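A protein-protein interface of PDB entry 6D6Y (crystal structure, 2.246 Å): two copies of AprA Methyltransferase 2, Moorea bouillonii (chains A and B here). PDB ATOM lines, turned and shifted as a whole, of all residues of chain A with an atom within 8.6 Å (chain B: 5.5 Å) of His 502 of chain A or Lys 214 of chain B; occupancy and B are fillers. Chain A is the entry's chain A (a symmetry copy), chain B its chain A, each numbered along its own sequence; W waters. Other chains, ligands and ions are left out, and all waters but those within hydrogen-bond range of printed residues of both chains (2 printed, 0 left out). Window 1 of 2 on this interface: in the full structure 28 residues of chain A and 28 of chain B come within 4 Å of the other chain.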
ATOM      1  N   GLU A 150      24.373  16.760 -18.493  1.00  0.00           N
ATOM      2  CA  GLU A 150      23.927  15.560 -17.800  1.00  0.00           C
ATOM      3  C   GLU A 150      22.416  15.617 -17.568  1.00  0.00           C
ATOM      4  O   GLU A 150      21.795  16.682 -17.670  1.00  0.00           O
ATOM      5  CB  GLU A 150      24.689  15.389 -16.470  1.00  0.00           C
ATOM      6  CG  GLU A 150      26.214  15.173 -16.639  1.00  0.00           C
ATOM      7  CD  GLU A 150      26.586  13.877 -17.374  1.00  0.00           C
ATOM      8  OE1 GLU A 150      25.988  12.829 -17.060  1.00  0.00           O
ATOM      9  OE2 GLU A 150      27.483  13.899 -18.258  1.00  0.00           O
ATOM     10  N   LEU A 151      21.830  14.458 -17.229  1.00  0.00           N
ATOM     11  CA  LEU A 151      20.368  14.330 -17.139  1.00  0.00           C
ATOM     12  C   LEU A 151      19.718  15.416 -16.295  1.00  0.00           C
ATOM     13  O   LEU A 151      18.639  15.914 -16.644  1.00  0.00           O
ATOM     14  CB  LEU A 151      19.972  12.974 -16.558  1.00  0.00           C
ATOM     15  CG  LEU A 151      20.121  11.795 -17.504  1.00  0.00           C
ATOM     16  CD1 LEU A 151      19.324  10.634 -16.926  1.00  0.00           C
ATOM     17  CD2 LEU A 151      19.613  12.191 -18.873  1.00  0.00           C
ATOM     18  N   PRO A 494      19.480   1.138 -30.478  1.00  0.00           N
ATOM     19  CA  PRO A 494      18.771   2.002 -29.518  1.00  0.00           C
ATOM     20  C   PRO A 494      19.563   3.260 -29.217  1.00  0.00           C
ATOM     21  O   PRO A 494      20.751   3.162 -28.887  1.00  0.00           O
ATOM     22  CB  PRO A 494      18.681   1.144 -28.253  1.00  0.00           C
ATOM     23  CG  PRO A 494      19.470  -0.130 -28.554  1.00  0.00           C
ATOM     24  CD  PRO A 494      20.248   0.086 -29.810  1.00  0.00           C
ATOM     25  N   GLY A 496      19.792   7.048 -27.081  1.00  0.00           N
ATOM     26  CA  GLY A 496      19.302   7.957 -26.071  1.00  0.00           C
ATOM     27  C   GLY A 496      20.097   9.235 -26.106  1.00  0.00           C
ATOM     28  O   GLY A 496      20.804   9.493 -27.074  1.00  0.00           O
ATOM     29  N   LEU A 497      19.970  10.051 -25.070  1.00  0.00           N
ATOM     30  CA  LEU A 497      20.819  11.221 -24.926  1.00  0.00           C
ATOM     31  C   LEU A 497      22.288  10.803 -24.799  1.00  0.00           C
ATOM     32  O   LEU A 497      22.582   9.695 -24.339  1.00  0.00           O
ATOM     33  CB  LEU A 497      20.368  12.013 -23.696  1.00  0.00           C
ATOM     34  CG  LEU A 497      19.054  12.764 -23.941  1.00  0.00           C
ATOM     35  CD1 LEU A 497      18.302  13.048 -22.651  1.00  0.00           C
ATOM     36  CD2 LEU A 497      19.340  14.057 -24.697  1.00  0.00           C
ATOM     37  N   PRO A 498      23.229  11.672 -25.198  1.00  0.00           N
ATOM     38  CA  PRO A 498      24.641  11.244 -25.222  1.00  0.00           C
ATOM     39  C   PRO A 498      25.145  10.761 -23.886  1.00  0.00           C
ATOM     40  O   PRO A 498      25.875   9.763 -23.841  1.00  0.00           O
ATOM     41  CB  PRO A 498      25.406  12.490 -25.685  1.00  0.00           C
ATOM     42  CG  PRO A 498      24.395  13.545 -25.943  1.00  0.00           C
ATOM     43  CD  PRO A 498      23.022  12.957 -25.871  1.00  0.00           C
ATOM     44  N   CYS A 499      24.732  11.411 -22.790  1.00  0.00           N
ATOM     45  CA  CYS A 499      25.200  11.096 -21.443  1.00  0.00           C
ATOM     46  C   CYS A 499      24.644   9.778 -20.899  1.00  0.00           C
ATOM     47  O   CYS A 499      25.025   9.375 -19.799  1.00  0.00           O
ATOM     48  CB  CYS A 499      24.844  12.237 -20.482  1.00  0.00           C
ATOM     49  SG  CYS A 499      23.053  12.442 -20.209  1.00  0.00           S
ATOM     50  N   GLU A 500      23.780   9.078 -21.627  1.00  0.00           N
ATOM     51  CA  GLU A 500      23.218   7.825 -21.136  1.00  0.00           C
ATOM     52  C   GLU A 500      23.322   6.692 -22.155  1.00  0.00           C
ATOM     53  O   GLU A 500      22.637   5.677 -22.008  1.00  0.00           O
ATOM     54  CB  GLU A 500      21.750   8.018 -20.732  1.00  0.00           C
ATOM     55  CG  GLU A 500      20.875   8.525 -21.851  1.00  0.00           C
ATOM     56  CD  GLU A 500      19.411   8.692 -21.452  1.00  0.00           C
ATOM     57  OE1 GLU A 500      19.051   8.379 -20.293  1.00  0.00           O
ATOM     58  OE2 GLU A 500      18.622   9.161 -22.303  1.00  0.00           O
ATOM     59  N   MET A 501      24.151   6.838 -23.195  1.00  0.00           N
ATOM     60  CA  MET A 501      24.286   5.757 -24.168  1.00  0.00           C
ATOM     61  C   MET A 501      24.751   4.465 -23.510  1.00  0.00           C
ATOM     62  O   MET A 501      24.474   3.379 -24.022  1.00  0.00           O
ATOM     63  CB  MET A 501      25.253   6.161 -25.278  1.00  0.00           C
ATOM     64  CG  MET A 501      24.668   7.145 -26.263  1.00  0.00           C
ATOM     65  SD  MET A 501      23.168   6.546 -27.054  1.00  0.00           S
ATOM     66  CE  MET A 501      23.857   5.229 -28.043  1.00  0.00           C
ATOM     67  N   HIS A 502      25.416   4.563 -22.364  1.00  0.00           N
ATOM     68  CA  HIS A 502      25.804   3.410 -21.560  1.00  0.00           C
ATOM     69  C   HIS A 502      24.754   2.989 -20.531  1.00  0.00           C
ATOM     70  O   HIS A 502      24.996   2.036 -19.784  1.00  0.00           O
ATOM     71  CB  HIS A 502      27.110   3.711 -20.824  1.00  0.00           C
ATOM     72  CG  HIS A 502      26.963   4.724 -19.735  1.00  0.00           C
ATOM     73  ND1 HIS A 502      26.574   6.022 -19.978  1.00  0.00           N
ATOM     74  CD2 HIS A 502      27.158   4.633 -18.397  1.00  0.00           C
ATOM     75  CE1 HIS A 502      26.532   6.687 -18.838  1.00  0.00           C
ATOM     76  NE2 HIS A 502      26.889   5.869 -17.864  1.00  0.00           N
ATOM     77  N   ALA A 503      23.608   3.668 -20.458  1.00  0.00           N
ATOM     78  CA  ALA A 503      22.616   3.413 -19.412  1.00  0.00           C
ATOM     79  C   ALA A 503      21.214   3.471 -19.986  1.00  0.00           C
ATOM     80  O   ALA A 503      20.293   4.029 -19.370  1.00  0.00           O
ATOM     81  CB  ALA A 503      22.751   4.412 -18.263  1.00  0.00           C
ATOM     82  N   LEU A 504      21.029   2.903 -21.186  1.00  0.00           N
ATOM     83  CA  LEU A 504      19.751   3.080 -21.868  1.00  0.00           C
ATOM     84  C   LEU A 504      18.611   2.289 -21.243  1.00  0.00           C
ATOM     85  O   LEU A 504      17.454   2.614 -21.495  1.00  0.00           O
ATOM     86  CB  LEU A 504      19.873   2.748 -23.359  1.00  0.00           C
ATOM     87  CG  LEU A 504      20.901   3.598 -24.111  1.00  0.00           C
ATOM     88  CD1 LEU A 504      21.301   2.972 -25.442  1.00  0.00           C
ATOM     89  CD2 LEU A 504      20.368   5.017 -24.313  1.00  0.00           C
ATOM     90  N   SER A 505      18.897   1.294 -20.408  1.00  0.00           N
ATOM     91  CA  SER A 505      17.830   0.575 -19.720  1.00  0.00           C
ATOM     92  C   SER A 505      17.014   1.482 -18.804  1.00  0.00           C
ATOM     93  O   SER A 505      15.934   1.084 -18.354  1.00  0.00           O
ATOM     94  CB  SER A 505      18.431  -0.574 -18.910  1.00  0.00           C
ATOM     95  OG  SER A 505      19.277  -0.037 -17.917  1.00  0.00           O
ATOM     96  N   LYS A 506      17.518   2.675 -18.493  1.00  0.00           N
ATOM     97  CA  LYS A 506      16.822   3.640 -17.657  1.00  0.00           C
ATOM     98  C   LYS A 506      16.427   4.899 -18.422  1.00  0.00           C
ATOM     99  O   LYS A 506      16.010   5.877 -17.794  1.00  0.00           O
ATOM    100  CB  LYS A 506      17.686   4.022 -16.449  1.00  0.00           C
ATOM    101  CG  LYS A 506      17.838   2.923 -15.408  1.00  0.00           C
ATOM    102  CD  LYS A 506      16.473   2.342 -15.062  1.00  0.00           C
ATOM    103  CE  LYS A 506      16.571   1.210 -14.049  1.00  0.00           C
ATOM    104  NZ  LYS A 506      15.273   0.480 -13.917  1.00  0.00           N
ATOM    105  N   ALA A 507      16.551   4.904 -19.753  1.00  0.00           N
ATOM    106  CA  ALA A 507      16.332   6.123 -20.527  1.00  0.00           C
ATOM    107  C   ALA A 507      14.843   6.430 -20.663  1.00  0.00           C
ATOM    108  O   ALA A 507      14.035   5.542 -20.938  1.00  0.00           O
ATOM    109  CB  ALA A 507      16.963   6.001 -21.922  1.00  0.00           C
ATOM    110  N   LEU B 209      39.126   3.188 -11.676  1.00  0.00           N
ATOM    111  CA  LEU B 209      38.599   2.561 -12.896  1.00  0.00           C
ATOM    112  C   LEU B 209      37.084   2.411 -12.814  1.00  0.00           C
ATOM    113  O   LEU B 209      36.372   2.595 -13.806  1.00  0.00           O
ATOM    114  CB  LEU B 209      39.250   1.186 -13.154  1.00  0.00           C
ATOM    115  CG  LEU B 209      40.763   1.084 -13.409  1.00  0.00           C
ATOM    116  CD1 LEU B 209      41.234  -0.355 -13.562  1.00  0.00           C
ATOM    117  CD2 LEU B 209      41.110   1.855 -14.652  1.00  0.00           C
ATOM    118  N   GLN B 210      36.577   2.088 -11.626  1.00  0.00           N
ATOM    119  CA  GLN B 210      35.139   1.918 -11.459  1.00  0.00           C
ATOM    120  C   GLN B 210      34.376   3.229 -11.705  1.00  0.00           C
ATOM    121  O   GLN B 210      33.296   3.215 -12.318  1.00  0.00           O
ATOM    122  CB  GLN B 210      34.861   1.341 -10.075  1.00  0.00           C
ATOM    123  CG  GLN B 210      33.410   1.246  -9.724  1.00  0.00           C
ATOM    124  CD  GLN B 210      32.693   0.181 -10.529  1.00  0.00           C
ATOM    125  OE1 GLN B 210      33.306  -0.567 -11.319  1.00  0.00           O
ATOM    126  NE2 GLN B 210      31.383   0.101 -10.331  1.00  0.00           N
ATOM    127  N   ILE B 211      34.925   4.373 -11.268  1.00  0.00           N
ATOM    128  CA  ILE B 211      34.317   5.666 -11.605  1.00  0.00           C
ATOM    129  C   ILE B 211      34.092   5.777 -13.109  1.00  0.00           C
ATOM    130  O   ILE B 211      32.980   6.060 -13.571  1.00  0.00           O
ATOM    131  CB  ILE B 211      35.187   6.833 -11.093  1.00  0.00           C
ATOM    132  CG1 ILE B 211      35.171   6.916  -9.570  1.00  0.00           C
ATOM    133  CG2 ILE B 211      34.761   8.187 -11.732  1.00  0.00           C
ATOM    134  CD1 ILE B 211      35.991   8.084  -9.036  1.00  0.00           C
ATOM    135  N   LEU B 212      35.153   5.556 -13.905  1.00  0.00           N
ATOM    136  CA  LEU B 212      34.990   5.640 -15.365  1.00  0.00           C
ATOM    137  C   LEU B 212      34.061   4.565 -15.916  1.00  0.00           C
ATOM    138  O   LEU B 212      33.383   4.795 -16.925  1.00  0.00           O
ATOM    139  CB  LEU B 212      36.338   5.565 -16.069  1.00  0.00           C
ATOM    140  CG  LEU B 212      37.301   6.617 -15.514  1.00  0.00           C
ATOM    141  CD1 LEU B 212      38.705   6.423 -16.095  1.00  0.00           C
ATOM    142  CD2 LEU B 212      36.732   7.999 -15.818  1.00  0.00           C
ATOM    143  N   HIS B 213      34.017   3.394 -15.279  1.00  0.00           N
ATOM    144  CA  HIS B 213      33.104   2.338 -15.706  1.00  0.00           C
ATOM    145  C   HIS B 213      31.647   2.801 -15.647  1.00  0.00           C
ATOM    146  O   HIS B 213      30.873   2.606 -16.596  1.00  0.00           O
ATOM    147  CB  HIS B 213      33.311   1.105 -14.823  1.00  0.00           C
ATOM    148  CG  HIS B 213      32.354  -0.015 -15.095  1.00  0.00           C
ATOM    149  ND1 HIS B 213      32.187  -0.577 -16.345  1.00  0.00           N
ATOM    150  CD2 HIS B 213      31.513  -0.686 -14.269  1.00  0.00           C
ATOM    151  CE1 HIS B 213      31.296  -1.554 -16.275  1.00  0.00           C
ATOM    152  NE2 HIS B 213      30.866  -1.634 -15.029  1.00  0.00           N
ATOM    153  N   LYS B 214      31.256   3.418 -14.531  1.00  0.00           N
ATOM    154  CA  LYS B 214      29.863   3.815 -14.356  1.00  0.00           C
ATOM    155  C   LYS B 214      29.481   4.986 -15.251  1.00  0.00           C
ATOM    156  O   LYS B 214      28.293   5.225 -15.453  1.00  0.00           O
ATOM    157  CB  LYS B 214      29.580   4.132 -12.880  1.00  0.00           C
ATOM    158  CG  LYS B 214      29.676   2.890 -11.986  1.00  0.00           C
ATOM    159  CD  LYS B 214      29.041   3.110 -10.628  1.00  0.00           C
ATOM    160  CE  LYS B 214      29.773   4.191  -9.837  1.00  0.00           C
ATOM    161  NZ  LYS B 214      30.552   3.692  -8.675  1.00  0.00           N
ATOM    162  N   ARG B 215      30.450   5.698 -15.815  1.00  0.00           N
ATOM    163  CA  ARG B 215      30.162   6.787 -16.729  1.00  0.00           C
ATOM    164  C   ARG B 215      30.323   6.386 -18.181  1.00  0.00           C
ATOM    165  O   ARG B 215      30.313   7.257 -19.064  1.00  0.00           O
ATOM    166  CB  ARG B 215      31.048   7.986 -16.388  1.00  0.00           C
ATOM    167  CG  ARG B 215      30.823   8.380 -14.951  1.00  0.00           C
ATOM    168  CD  ARG B 215      31.254   9.761 -14.625  1.00  0.00           C
ATOM    169  NE  ARG B 215      30.944  10.043 -13.235  1.00  0.00           N
ATOM    170  CZ  ARG B 215      30.011  10.901 -12.830  1.00  0.00           C
ATOM    171  NH1 ARG B 215      29.288  11.587 -13.725  1.00  0.00           N
ATOM    172  NH2 ARG B 215      29.812  11.078 -11.524  1.00  0.00           N
ATOM    173  N   GLY B 216      30.442   5.092 -18.456  1.00  0.00           N
ATOM    174  CA  GLY B 216      30.459   4.626 -19.832  1.00  0.00           C
ATOM    175  C   GLY B 216      31.771   4.808 -20.550  1.00  0.00           C
ATOM    176  O   GLY B 216      31.809   4.668 -21.775  1.00  0.00           O
ATOM    177  N   LEU B 218      34.733   3.104 -19.702  1.00  0.00           N
ATOM    178  CA  LEU B 218      35.351   1.790 -19.711  1.00  0.00           C
ATOM    179  C   LEU B 218      34.272   0.731 -19.534  1.00  0.00           C
ATOM    180  O   LEU B 218      33.237   0.980 -18.912  1.00  0.00           O
ATOM    181  CB  LEU B 218      36.367   1.635 -18.561  1.00  0.00           C
ATOM    182  CG  LEU B 218      37.444   2.677 -18.293  1.00  0.00           C
ATOM    183  CD1 LEU B 218      38.199   2.279 -17.040  1.00  0.00           C
ATOM    184  CD2 LEU B 218      38.400   2.822 -19.493  1.00  0.00           C
ATOM    185  N   ARG B 230      33.259   6.289 -26.001  1.00  0.00           N
ATOM    186  CA  ARG B 230      33.068   7.575 -25.345  1.00  0.00           C
ATOM    187  C   ARG B 230      34.369   8.129 -24.786  1.00  0.00           C
ATOM    188  O   ARG B 230      34.467   9.342 -24.557  1.00  0.00           O
ATOM    189  CB  ARG B 230      32.017   7.434 -24.235  1.00  0.00           C
ATOM    190  CG  ARG B 230      31.230   8.712 -23.932  1.00  0.00           C
ATOM    191  CD  ARG B 230      30.645   8.728 -22.508  1.00  0.00           C
ATOM    192  NE  ARG B 230      29.883   9.948 -22.255  1.00  0.00           N
ATOM    193  CZ  ARG B 230      29.376  10.283 -21.070  1.00  0.00           C
ATOM    194  NH1 ARG B 230      29.557   9.494 -20.023  1.00  0.00           N
ATOM    195  NH2 ARG B 230      28.689  11.408 -20.925  1.00  0.00           N
ATOM    196  N   PRO B 445      28.646   4.359  -3.103  1.00  0.00           N
ATOM    197  CA  PRO B 445      30.087   4.507  -3.451  1.00  0.00           C
ATOM    198  C   PRO B 445      30.327   5.744  -4.311  1.00  0.00           C
ATOM    199  O   PRO B 445      30.636   5.636  -5.495  1.00  0.00           O
ATOM    200  CB  PRO B 445      30.368   3.200  -4.192  1.00  0.00           C
ATOM    201  CG  PRO B 445      29.056   2.930  -4.935  1.00  0.00           C
ATOM    202  CD  PRO B 445      27.936   3.440  -4.066  1.00  0.00           C
ATOM    203  N   ASP B 447      31.669   9.057  -6.160  1.00  0.00           N
ATOM    204  CA  ASP B 447      32.961   9.434  -6.742  1.00  0.00           C
ATOM    205  C   ASP B 447      33.668  10.470  -5.876  1.00  0.00           C
ATOM    206  O   ASP B 447      34.850  10.317  -5.548  1.00  0.00           O
ATOM    207  CB  ASP B 447      32.818  10.016  -8.158  1.00  0.00           C
ATOM    208  CG  ASP B 447      32.163   9.086  -9.143  1.00  0.00           C
ATOM    209  OD1 ASP B 447      31.754   9.582 -10.224  1.00  0.00           O
ATOM    210  OD2 ASP B 447      32.012   7.890  -8.830  1.00  0.00           O
ATOM    211  N   GLU B 470      30.470  -2.102  -3.866  1.00  0.00           N
ATOM    212  CA  GLU B 470      31.370  -2.110  -5.017  1.00  0.00           C
ATOM    213  C   GLU B 470      32.815  -2.449  -4.652  1.00  0.00           C
ATOM    214  O   GLU B 470      33.110  -3.560  -4.207  1.00  0.00           O
ATOM    215  CB  GLU B 470      31.337  -0.750  -5.711  1.00  0.00           C
ATOM    216  CG  GLU B 470      30.024  -0.378  -6.365  1.00  0.00           C
ATOM    217  CD  GLU B 470      30.174   0.853  -7.252  1.00  0.00           C
ATOM    218  OE1 GLU B 470      31.286   1.424  -7.284  1.00  0.00           O
ATOM    219  OE2 GLU B 470      29.192   1.240  -7.923  1.00  0.00           O
HETATM  220  O   HOH W   1      27.343   7.552 -22.354  1.00  0.00           O
HETATM  221  O   HOH W   2      26.437   7.822 -15.699  1.00  0.00           O
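Of the printed residues of chain B, Glu 150 of chain A touches Arg 230 (3.8 Å).
Of the printed residues of chain B, Cys 499 of chain A touches Arg 230 (3.5 Å).
His 502 of chain A touches three residues of chain B.
Ser 505 of chain A touches none of the printed residues of chain B.
Lys 214 of chain B touches just one residue of chain A: His 502.
The nearest residue of chain B that does not touch His 502 of chain A is Arg 230 of chain B (4.3 Å).
The nearest printed residue of chain A that does not touch Arg 230 of chain B is His 502 of chain A (4.3 Å).
No position is printed for both chains.
O of Lys 214 of chain B sits at hydrogen-bond distance from NE2 of His 502 of chain A (2.9 Å).
The guanidinium group (NH2) of Arg 230 of chain B lies within salt-bridge range of the side-chain carboxylate (OE2) of Glu 150 of chain A.
Among the printed residues, merely in contact across the chains: Cys 499 of chain A with Arg 230 of chain B (3.5 Å), His 502 of chain A with Arg 215 of chain B (3.5 Å) and His 502 of chain A with Gly 216 of chain B (3.3 Å).
Water W1 lies within hydrogen-bond range of a ring nitrogen (ND1) of His 502 of chain A (2.9 Å), the backbone carbonyl oxygen (O) of Pro 498 of chain A (3.0 Å), the backbone NH (N) of Met 501 of chain A (3.4 Å) and the guanidinium group (NE) of Arg 230 of chain B (3.5 Å).
Water W2 bridges a ring nitrogen (NE2) of His 502 of chain A (3.0 Å) and the backbone carbonyl oxygen (O) of Lys 214 of chain B (3.2 Å).
Printed residues of chain A that touch a printed residue of chain B: Glu 150, Cys 499 and His 502.
Hydrophobic or aromatic side chains of chain A that line the printed part of chain B: His 502.
Of the 13 printed residues of chain B, 4 touch a printed residue of chain A.
Along chain B the printed residues that touch a printed residue of chain A span positions 214 to 230.
Among the printed residues, Asp or Glu carboxylates within 4 Å of a Lys or Arg side-chain nitrogen of the other chain: Glu 150 of chain A with Arg 230 of chain B.
The side-chain amino group of Lys 214 of chain B is in salt-bridge range of the side-chain carboxylate of Glu 470 of chain B (2.8 Å).
The backbone NH (N) of Leu 151 of chain A lies close to the side-chain sulfur (SG) of Cys 499 of chain A (3.8 Å).
NH2 of Arg 215 of chain B lies within salt-bridge range of OD1 of Asp 447 of chain B.
NH1 of Arg 230 of chain B sits at hydrogen-bond distance from O of Arg 215 of chain B.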
